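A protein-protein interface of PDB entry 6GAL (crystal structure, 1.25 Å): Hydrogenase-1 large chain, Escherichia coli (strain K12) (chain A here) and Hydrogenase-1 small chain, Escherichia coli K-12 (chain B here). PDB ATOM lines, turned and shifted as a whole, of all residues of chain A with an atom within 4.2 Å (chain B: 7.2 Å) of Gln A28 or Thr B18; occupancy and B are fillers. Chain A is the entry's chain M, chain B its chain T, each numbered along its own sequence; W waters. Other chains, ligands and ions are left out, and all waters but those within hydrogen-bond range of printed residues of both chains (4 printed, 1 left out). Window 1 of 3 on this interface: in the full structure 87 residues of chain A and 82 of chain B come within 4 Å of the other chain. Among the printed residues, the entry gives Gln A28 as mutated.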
ATOM      1  N   ILE A  27     -25.407   8.506  27.834  1.00  0.00           N
ATOM      2  CA  ILE A  27     -26.084   7.435  27.118  1.00  0.00           C
ATOM      3  C   ILE A  27     -26.464   7.990  25.769  1.00  0.00           C
ATOM      4  O   ILE A  27     -26.352   9.208  25.550  1.00  0.00           O
ATOM      5  CB  ILE A  27     -27.338   6.922  27.837  1.00  0.00           C
ATOM      6  CG1 ILE A  27     -28.390   8.047  27.961  1.00  0.00           C
ATOM      7  CG2 ILE A  27     -27.006   6.343  29.188  1.00  0.00           C
ATOM      8  CD1 ILE A  27     -29.762   7.613  28.407  1.00  0.00           C
ATOM      9  N   GLN A  28     -26.935   7.131  24.870  1.00  0.00           N
ATOM     10  CA  GLN A  28     -27.604   7.594  23.661  1.00  0.00           C
ATOM     11  C   GLN A  28     -29.073   7.776  23.952  1.00  0.00           C
ATOM     12  O   GLN A  28     -29.704   6.917  24.580  1.00  0.00           O
ATOM     13  CB  GLN A  28     -27.440   6.599  22.510  1.00  0.00           C
ATOM     14  CG  GLN A  28     -27.905   7.173  21.162  1.00  0.00           C
ATOM     15  CD  GLN A  28     -29.406   7.402  21.025  1.00  0.00           C
ATOM     16  OE1 GLN A  28     -30.143   6.603  21.605  1.00  0.00           O
ATOM     17  NE2 GLN A  28     -29.880   8.468  20.234  1.00  0.00           N
ATOM     18  N   GLY A  29     -29.617   8.869  23.457  1.00  0.00           N
ATOM     19  CA  GLY A  29     -31.065   9.086  23.505  1.00  0.00           C
ATOM     20  C   GLY A  29     -31.529   9.595  24.855  1.00  0.00           C
ATOM     21  O   GLY A  29     -30.785  10.248  25.573  1.00  0.00           O
ATOM     22  N   HIS A  30     -32.793   9.368  25.134  1.00  0.00           N
ATOM     23  CA  HIS A  30     -33.457   9.979  26.277  1.00  0.00           C
ATOM     24  C   HIS A  30     -33.976   8.904  27.233  1.00  0.00           C
ATOM     25  O   HIS A  30     -34.738   8.031  26.820  1.00  0.00           O
ATOM     26  CB  HIS A  30     -34.614  10.847  25.770  1.00  0.00           C
ATOM     27  CG  HIS A  30     -34.142  12.001  24.924  1.00  0.00           C
ATOM     28  ND1 HIS A  30     -33.489  13.101  25.452  1.00  0.00           N
ATOM     29  CD2 HIS A  30     -34.148  12.175  23.582  1.00  0.00           C
ATOM     30  CE1 HIS A  30     -33.196  13.921  24.467  1.00  0.00           C
ATOM     31  NE2 HIS A  30     -33.571  13.374  23.321  1.00  0.00           N
ATOM     32  N   VAL A  78     -25.103   5.393  16.855  1.00  0.00           N
ATOM     33  CA  VAL A  78     -24.070   4.897  17.733  1.00  0.00           C
ATOM     34  C   VAL A  78     -23.786   3.413  17.374  1.00  0.00           C
ATOM     35  O   VAL A  78     -22.645   3.065  16.956  1.00  0.00           O
ATOM     36  CB  VAL A  78     -24.376   5.096  19.213  1.00  0.00           C
ATOM     37  CG1 VAL A  78     -23.201   4.599  20.029  1.00  0.00           C
ATOM     38  CG2 VAL A  78     -24.651   6.572  19.522  1.00  0.00           C
ATOM     39  N   PRO A 575     -26.577   1.876  27.682  1.00  0.00           N
ATOM     40  CA  PRO A 575     -27.939   2.147  27.184  1.00  0.00           C
ATOM     41  C   PRO A 575     -27.989   2.920  25.862  1.00  0.00           C
ATOM     42  O   PRO A 575     -27.404   3.975  25.734  1.00  0.00           O
ATOM     43  CB  PRO A 575     -28.587   2.942  28.312  1.00  0.00           C
ATOM     44  CG  PRO A 575     -27.778   2.623  29.506  1.00  0.00           C
ATOM     45  CD  PRO A 575     -26.370   2.506  29.009  1.00  0.00           C
ATOM     46  N   CYS A 576     -28.846   2.411  24.970  1.00  0.00           N
ATOM     47  CA  CYS A 576     -29.101   3.068  23.712  1.00  0.00           C
ATOM     48  C   CYS A 576     -30.618   3.272  23.588  1.00  0.00           C
ATOM     49  O   CYS A 576     -31.365   2.337  23.254  1.00  0.00           O
ATOM     50  CB  CYS A 576     -28.568   2.251  22.534  1.00  0.00           C
ATOM     51  SG  CYS A 576     -28.602   3.236  21.048  1.00  0.00           S
ATOM     52  N   LEU A 577     -31.071   4.463  23.916  1.00  0.00           N
ATOM     53  CA  LEU A 577     -32.500   4.658  24.076  1.00  0.00           C
ATOM     54  C   LEU A 577     -33.230   4.822  22.762  1.00  0.00           C
ATOM     55  O   LEU A 577     -34.404   4.439  22.663  1.00  0.00           O
ATOM     56  CB  LEU A 577     -32.810   5.809  25.051  1.00  0.00           C
ATOM     57  CG  LEU A 577     -32.728   5.400  26.544  1.00  0.00           C
ATOM     58  CD1 LEU A 577     -33.969   4.608  26.948  1.00  0.00           C
ATOM     59  CD2 LEU A 577     -31.502   4.619  26.947  1.00  0.00           C
ATOM     60  N   ALA A 578     -32.587   5.387  21.748  1.00  0.00           N
ATOM     61  CA  ALA A 578     -33.153   5.456  20.415  1.00  0.00           C
ATOM     62  C   ALA A 578     -33.306   4.065  19.850  1.00  0.00           C
ATOM     63  O   ALA A 578     -34.332   3.745  19.218  1.00  0.00           O
ATOM     64  CB  ALA A 578     -32.330   6.322  19.507  1.00  0.00           C
ATOM     65  N   HIS B  13     -30.342  17.815  22.331  1.00  0.00           N
ATOM     66  CA  HIS B  13     -30.798  16.674  21.540  1.00  0.00           C
ATOM     67  C   HIS B  13     -32.303  16.491  21.634  1.00  0.00           C
ATOM     68  O   HIS B  13     -32.812  16.297  22.754  1.00  0.00           O
ATOM     69  CB  HIS B  13     -30.117  15.382  22.045  1.00  0.00           C
ATOM     70  CG  HIS B  13     -28.652  15.342  21.843  1.00  0.00           C
ATOM     71  ND1 HIS B  13     -27.780  15.928  22.728  1.00  0.00           N
ATOM     72  CD2 HIS B  13     -27.892  14.724  20.901  1.00  0.00           C
ATOM     73  CE1 HIS B  13     -26.546  15.704  22.309  1.00  0.00           C
ATOM     74  NE2 HIS B  13     -26.577  14.986  21.193  1.00  0.00           N
ATOM     75  N   GLY B  14     -32.993  16.530  20.509  1.00  0.00           N
ATOM     76  CA  GLY B  14     -34.390  16.199  20.434  1.00  0.00           C
ATOM     77  C   GLY B  14     -34.594  14.739  20.077  1.00  0.00           C
ATOM     78  O   GLY B  14     -33.899  13.894  20.601  1.00  0.00           O
ATOM     79  N   LEU B  15     -35.523  14.459  19.161  1.00  0.00           N
ATOM     80  CA  LEU B  15     -35.611  13.142  18.551  1.00  0.00           C
ATOM     81  C   LEU B  15     -34.483  13.011  17.544  1.00  0.00           C
ATOM     82  O   LEU B  15     -34.393  13.825  16.637  1.00  0.00           O
ATOM     83  CB  LEU B  15     -36.923  12.951  17.849  1.00  0.00           C
ATOM     84  CG  LEU B  15     -38.166  12.844  18.735  1.00  0.00           C
ATOM     85  CD1 LEU B  15     -39.396  12.633  17.858  1.00  0.00           C
ATOM     86  CD2 LEU B  15     -38.055  11.723  19.760  1.00  0.00           C
ATOM     87  N   GLU B  16     -33.631  11.991  17.707  1.00  0.00           N
ATOM     88  CA  GLU B  16     -32.399  11.845  16.934  1.00  0.00           C
ATOM     89  C   GLU B  16     -31.799  10.479  17.203  1.00  0.00           C
ATOM     90  O   GLU B  16     -32.148   9.792  18.183  1.00  0.00           O
ATOM     91  CB  GLU B  16     -31.394  12.945  17.253  1.00  0.00           C
ATOM     92  CG  GLU B  16     -31.191  13.341  18.696  1.00  0.00           C
ATOM     93  CD  GLU B  16     -30.192  12.491  19.458  1.00  0.00           C
ATOM     94  OE1 GLU B  16     -30.450  12.141  20.660  1.00  0.00           O
ATOM     95  OE2 GLU B  16     -29.121  12.154  18.866  1.00  0.00           O
ATOM     96  N   CYS B  17     -30.868  10.097  16.295  1.00  0.00           N
ATOM     97  CA  CYS B  17     -30.185   8.819  16.394  1.00  0.00           C
ATOM     98  C   CYS B  17     -28.750   8.958  16.916  1.00  0.00           C
ATOM     99  O   CYS B  17     -28.068   7.953  17.105  1.00  0.00           O
ATOM    100  CB  CYS B  17     -30.239   8.068  15.060  1.00  0.00           C
ATOM    101  SG  CYS B  17     -28.906   8.533  13.923  1.00  0.00           S
ATOM    102  N   THR B  18     -28.280  10.204  17.073  1.00  0.00           N
ATOM    103  CA  THR B  18     -26.924  10.561  17.484  1.00  0.00           C
ATOM    104  C   THR B  18     -25.883  10.473  16.375  1.00  0.00           C
ATOM    105  O   THR B  18     -24.720  10.614  16.649  1.00  0.00           O
ATOM    106  CB  THR B  18     -26.598   9.893  18.814  1.00  0.00           C
ATOM    107  OG1 THR B  18     -27.738  10.105  19.681  1.00  0.00           O
ATOM    108  CG2 THR B  18     -25.331  10.474  19.456  1.00  0.00           C
ATOM    109  N   CYS B  19     -26.333  10.284  15.135  1.00  0.00           N
ATOM    110  CA  CYS B  19     -25.372  10.258  14.030  1.00  0.00           C
ATOM    111  C   CYS B  19     -24.622  11.544  13.902  1.00  0.00           C
ATOM    112  O   CYS B  19     -23.490  11.523  13.448  1.00  0.00           O
ATOM    113  CB  CYS B  19     -25.950   9.810  12.706  1.00  0.00           C
ATOM    114  SG  CYS B  19     -27.277  10.778  11.868  1.00  0.00           S
ATOM    115  N   CYS B  20     -25.227  12.664  14.251  1.00  0.00           N
ATOM    116  CA  CYS B  20     -24.543  13.948  14.077  1.00  0.00           C
ATOM    117  C   CYS B  20     -23.464  14.184  15.131  1.00  0.00           C
ATOM    118  O   CYS B  20     -22.348  14.628  14.815  1.00  0.00           O
ATOM    119  CB  CYS B  20     -25.589  15.044  13.987  1.00  0.00           C
ATOM    120  SG  CYS B  20     -26.714  14.914  12.562  1.00  0.00           S
ATOM    121  N   THR B  21     -23.753  13.841  16.379  1.00  0.00           N
ATOM    122  CA  THR B  21     -22.697  13.822  17.418  1.00  0.00           C
ATOM    123  C   THR B  21     -21.561  12.891  17.028  1.00  0.00           C
ATOM    124  O   THR B  21     -20.377  13.211  17.197  1.00  0.00           O
ATOM    125  CB  THR B  21     -23.304  13.400  18.770  1.00  0.00           C
ATOM    126  OG1 THR B  21     -24.019  14.525  19.314  1.00  0.00           O
ATOM    127  CG2 THR B  21     -22.285  12.914  19.764  1.00  0.00           C
ATOM    128  N   GLU B  22     -21.914  11.705  16.590  1.00  0.00           N
ATOM    129  CA  GLU B  22     -20.900  10.703  16.215  1.00  0.00           C
ATOM    130  C   GLU B  22     -20.059  11.224  15.062  1.00  0.00           C
ATOM    131  O   GLU B  22     -18.843  11.088  15.094  1.00  0.00           O
ATOM    132  CB  GLU B  22     -21.555   9.368  15.878  1.00  0.00           C
ATOM    133  CG  GLU B  22     -22.078   8.654  17.088  1.00  0.00           C
ATOM    134  CD  GLU B  22     -20.993   8.084  17.989  1.00  0.00           C
ATOM    135  OE1 GLU B  22     -19.860   7.783  17.623  1.00  0.00           O
ATOM    136  OE2 GLU B  22     -21.307   7.849  19.151  1.00  0.00           O
ATOM    137  N   SER B  23     -20.672  11.854  14.080  1.00  0.00           N
ATOM    138  CA  SER B  23     -19.918  12.429  12.989  1.00  0.00           C
ATOM    139  C   SER B  23     -18.956  13.490  13.508  1.00  0.00           C
ATOM    140  O   SER B  23     -17.758  13.473  13.150  1.00  0.00           O
ATOM    141  CB  SER B  23     -20.871  13.053  11.971  1.00  0.00           C
ATOM    142  OG  SER B  23     -20.066  13.556  10.891  1.00  0.00           O
ATOM    143  N   PHE B  24     -19.415  14.354  14.402  1.00  0.00           N
ATOM    144  CA  PHE B  24     -18.548  15.393  14.959  1.00  0.00           C
ATOM    145  C   PHE B  24     -17.274  14.795  15.558  1.00  0.00           C
ATOM    146  O   PHE B  24     -16.177  15.305  15.316  1.00  0.00           O
ATOM    147  CB  PHE B  24     -19.339  16.244  15.960  1.00  0.00           C
ATOM    148  CG  PHE B  24     -18.491  17.163  16.807  1.00  0.00           C
ATOM    149  CD1 PHE B  24     -17.786  18.160  16.264  1.00  0.00           C
ATOM    150  CD2 PHE B  24     -18.389  16.938  18.169  1.00  0.00           C
ATOM    151  CE1 PHE B  24     -17.006  18.986  17.056  1.00  0.00           C
ATOM    152  CE2 PHE B  24     -17.596  17.711  18.958  1.00  0.00           C
ATOM    153  CZ  PHE B  24     -16.906  18.739  18.394  1.00  0.00           C
ATOM    154  N   ARG B  26     -15.742  12.187  14.802  1.00  0.00           N
ATOM    155  CA  ARG B  26     -14.837  11.655  13.789  1.00  0.00           C
ATOM    156  C   ARG B  26     -13.914  12.690  13.210  1.00  0.00           C
ATOM    157  O   ARG B  26     -13.034  12.312  12.439  1.00  0.00           O
ATOM    158  CB  ARG B  26     -15.611  11.030  12.631  1.00  0.00           C
ATOM    159  CG  ARG B  26     -16.600   9.922  12.979  1.00  0.00           C
ATOM    160  CD  ARG B  26     -15.987   8.730  13.643  1.00  0.00           C
ATOM    161  NE  ARG B  26     -17.061   7.709  13.788  1.00  0.00           N
ATOM    162  CZ  ARG B  26     -17.907   7.603  14.806  1.00  0.00           C
ATOM    163  NH1 ARG B  26     -17.686   8.190  15.999  1.00  0.00           N
ATOM    164  NH2 ARG B  26     -18.971   6.870  14.607  1.00  0.00           N
ATOM    165  N   ASP B  46     -25.576  16.240  26.456  1.00  0.00           N
ATOM    166  CA  ASP B  46     -26.030  15.033  27.177  1.00  0.00           C
ATOM    167  C   ASP B  46     -25.205  13.779  26.867  1.00  0.00           C
ATOM    168  O   ASP B  46     -25.185  12.870  27.678  1.00  0.00           O
ATOM    169  CB  ASP B  46     -27.511  14.719  26.858  1.00  0.00           C
ATOM    170  CG  ASP B  46     -28.509  15.629  27.564  1.00  0.00           C
ATOM    171  OD1 ASP B  46     -28.123  16.374  28.510  1.00  0.00           O
ATOM    172  OD2 ASP B  46     -29.699  15.516  27.209  1.00  0.00           O
ATOM    173  N   THR B  47     -24.603  13.692  25.669  1.00  0.00           N
ATOM    174  CA  THR B  47     -23.852  12.494  25.278  1.00  0.00           C
ATOM    175  C   THR B  47     -22.497  12.363  25.980  1.00  0.00           C
ATOM    176  O   THR B  47     -22.037  11.262  26.157  1.00  0.00           O
ATOM    177  CB  THR B  47     -23.701  12.371  23.743  1.00  0.00           C
ATOM    178  OG1 THR B  47     -22.835  13.371  23.249  1.00  0.00           O
ATOM    179  CG2 THR B  47     -25.037  12.445  23.096  1.00  0.00           C
ATOM    180  N   GLU B  76     -29.265  18.967  17.687  1.00  0.00           N
ATOM    181  CA  GLU B  76     -29.326  17.692  17.009  1.00  0.00           C
ATOM    182  C   GLU B  76     -30.685  17.098  17.234  1.00  0.00           C
ATOM    183  O   GLU B  76     -31.226  17.175  18.333  1.00  0.00           O
ATOM    184  CB  GLU B  76     -28.236  16.785  17.571  1.00  0.00           C
ATOM    185  CG  GLU B  76     -28.088  15.411  16.966  1.00  0.00           C
ATOM    186  CD  GLU B  76     -26.785  14.759  17.392  1.00  0.00           C
ATOM    187  OE1 GLU B  76     -26.498  13.645  16.889  1.00  0.00           O
ATOM    188  OE2 GLU B  76     -26.033  15.400  18.155  1.00  0.00           O
ATOM    189  N   GLY B  77     -31.279  16.596  16.180  1.00  0.00           N
ATOM    190  CA  GLY B  77     -32.631  16.106  16.267  1.00  0.00           C
ATOM    191  C   GLY B  77     -33.684  17.198  16.173  1.00  0.00           C
ATOM    192  O   GLY B  77     -33.401  18.352  15.829  1.00  0.00           O
ATOM    193  N   CYS B 115     -32.033  15.920  10.469  1.00  0.00           N
ATOM    194  CA  CYS B 115     -33.079  16.018  11.478  1.00  0.00           C
ATOM    195  C   CYS B 115     -33.405  17.460  11.845  1.00  0.00           C
ATOM    196  O   CYS B 115     -34.569  17.854  11.802  1.00  0.00           O
ATOM    197  CB  CYS B 115     -32.786  15.315  12.820  1.00  0.00           C
ATOM    198  SG  CYS B 115     -32.845  13.520  12.831  1.00  0.00           S
ATOM    199  N   PRO B 150     -25.379  11.517   8.625  1.00  0.00           N
ATOM    200  CA  PRO B 150     -25.149  12.869   9.143  1.00  0.00           C
ATOM    201  C   PRO B 150     -24.350  13.713   8.155  1.00  0.00           C
ATOM    202  O   PRO B 150     -23.914  13.202   7.130  1.00  0.00           O
ATOM    203  CB  PRO B 150     -24.294  12.579  10.401  1.00  0.00           C
ATOM    204  CG  PRO B 150     -23.476  11.389   9.991  1.00  0.00           C
ATOM    205  CD  PRO B 150     -24.274  10.600   8.989  1.00  0.00           C
HETATM  206  O   HOH W   1     -33.051  11.205  20.739  1.00  0.00           O
HETATM  207  O   HOH W   2     -30.697  13.076  26.783  1.00  0.00           O
HETATM  208  O   HOH W   3     -28.428  11.135  22.116  1.00  0.00           O
HETATM  209  O   HOH W   4     -21.070   5.440  15.811  1.00  0.00           O
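Water W2 lies within hydrogen-bond range of the side-chain carboxylate (OD2) of Asp B46 (2.7 Å), the backbone carbonyl oxygen (O) of Gly A29 (3.1 Å) and a ring nitrogen (ND1) of His A30 (3.1 Å). Water W3 lies within hydrogen-bond range of OE1 of Glu B16 (2.7 Å), OG1 of Thr B18 (2.7 Å) and N of Gly A29 (2.9 Å). Water W1 lies within hydrogen-bond range of OE1 of Glu B16 (2.8 Å), O of Gly B14 (2.8 Å) and NE2 of His A30 (3.4 Å). Water W4 lies within hydrogen-bond range of NH2 of Arg B26, O of Val A78 and OE1 of Glu B22.
A ring nitrogen (NE2) of His A30 lies close to the backbone carbonyl oxygen of His B13, at 3.1 Å. The backbone carbonyl oxygen (O) of Gly B14 lies within hydrogen-bond range of a ring nitrogen (NE2) of His A30, 2.8 Å away. The backbone carbonyl oxygen of Glu B16 is in hydrogen-bond range of the side-chain amide nitrogen of Gln A28 (3.3 Å). The side-chain hydroxyl (OG1) of Thr B18 is in hydrogen-bond range of the side-chain amide nitrogen (NE2) of Gln A28, 2.8 Å away.
O of Glu B76 lies within hydrogen-bond range of N of Gly B14 (2.9 Å). The side-chain hydroxyl (OG1) of Thr B18 lies within hydrogen-bond range of the side-chain carboxylate (OE2) of Glu B16 (2.6 Å). The side-chain carboxylate of Glu B22 lies within salt-bridge range of the guanidinium group of Arg B26 (2.7 Å). The backbone NH (N) of Gln A28 lies within hydrogen-bond range of the backbone carbonyl oxygen (O) of Pro A575 (3.3 Å). The side-chain amide oxygen (OE1) of Gln A28 sits close to the side-chain sulfur (SG) of Cys A576 (3.7 Å). The side-chain amide oxygen of Gln A28 is in hydrogen-bond range of the backbone NH of Ala A578.
Gln A28 touches just these residues of chain B: Glu B16 (3.3 Å), Cys B17 (3.5 Å) and Thr B18 (2.8 Å). Of the printed residues of chain B, Ala A578 touches Glu B16 (3.7 Å). Printed residues of chain A within 4 Å of His B13: His A30 (3.0 Å). Printed residues of chain A within 4 Å of Cys B17: Gln A28 (3.5 Å) and Val A78 (3.9 Å). Thr B18 touches two residues of chain A. Of the printed residues of chain A, Glu B22 touches Val A78. Arg B26 touches none of the printed residues of chain A. The nearest residue of chain B that does not touch Gln A28 is Thr B47 (5.5 Å). The nearest printed residue of chain A that does not touch Glu B22 is Gln A28 (6.9 Å).
Of the 19 printed residues of chain B, 6 touch a printed residue of chain A. Of the 9 printed residues of chain A, 4 touch a printed residue of chain B. Hydrophobic or aromatic side chains of chain A within 4 Å of the printed part of chain B: His A30, Val A78 and Ala A578. Along chain A the printed residues that touch a printed residue of chain B span positions 28 to 578. Among the printed residues, no Asp or Glu carboxylate lies within 4 Å of a Lys or Arg side-chain nitrogen of the other chain.
NE2 of Gln A28 touches C of Cys B17, 3.5 Å away. Val A78 touches Cys B17 (N to O, 3.9 Å). Val A78 touches Thr B18. Val A78 touches Glu B22 (CG2 to OE2, 3.6 Å). Glu B16 touches Ala A578.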
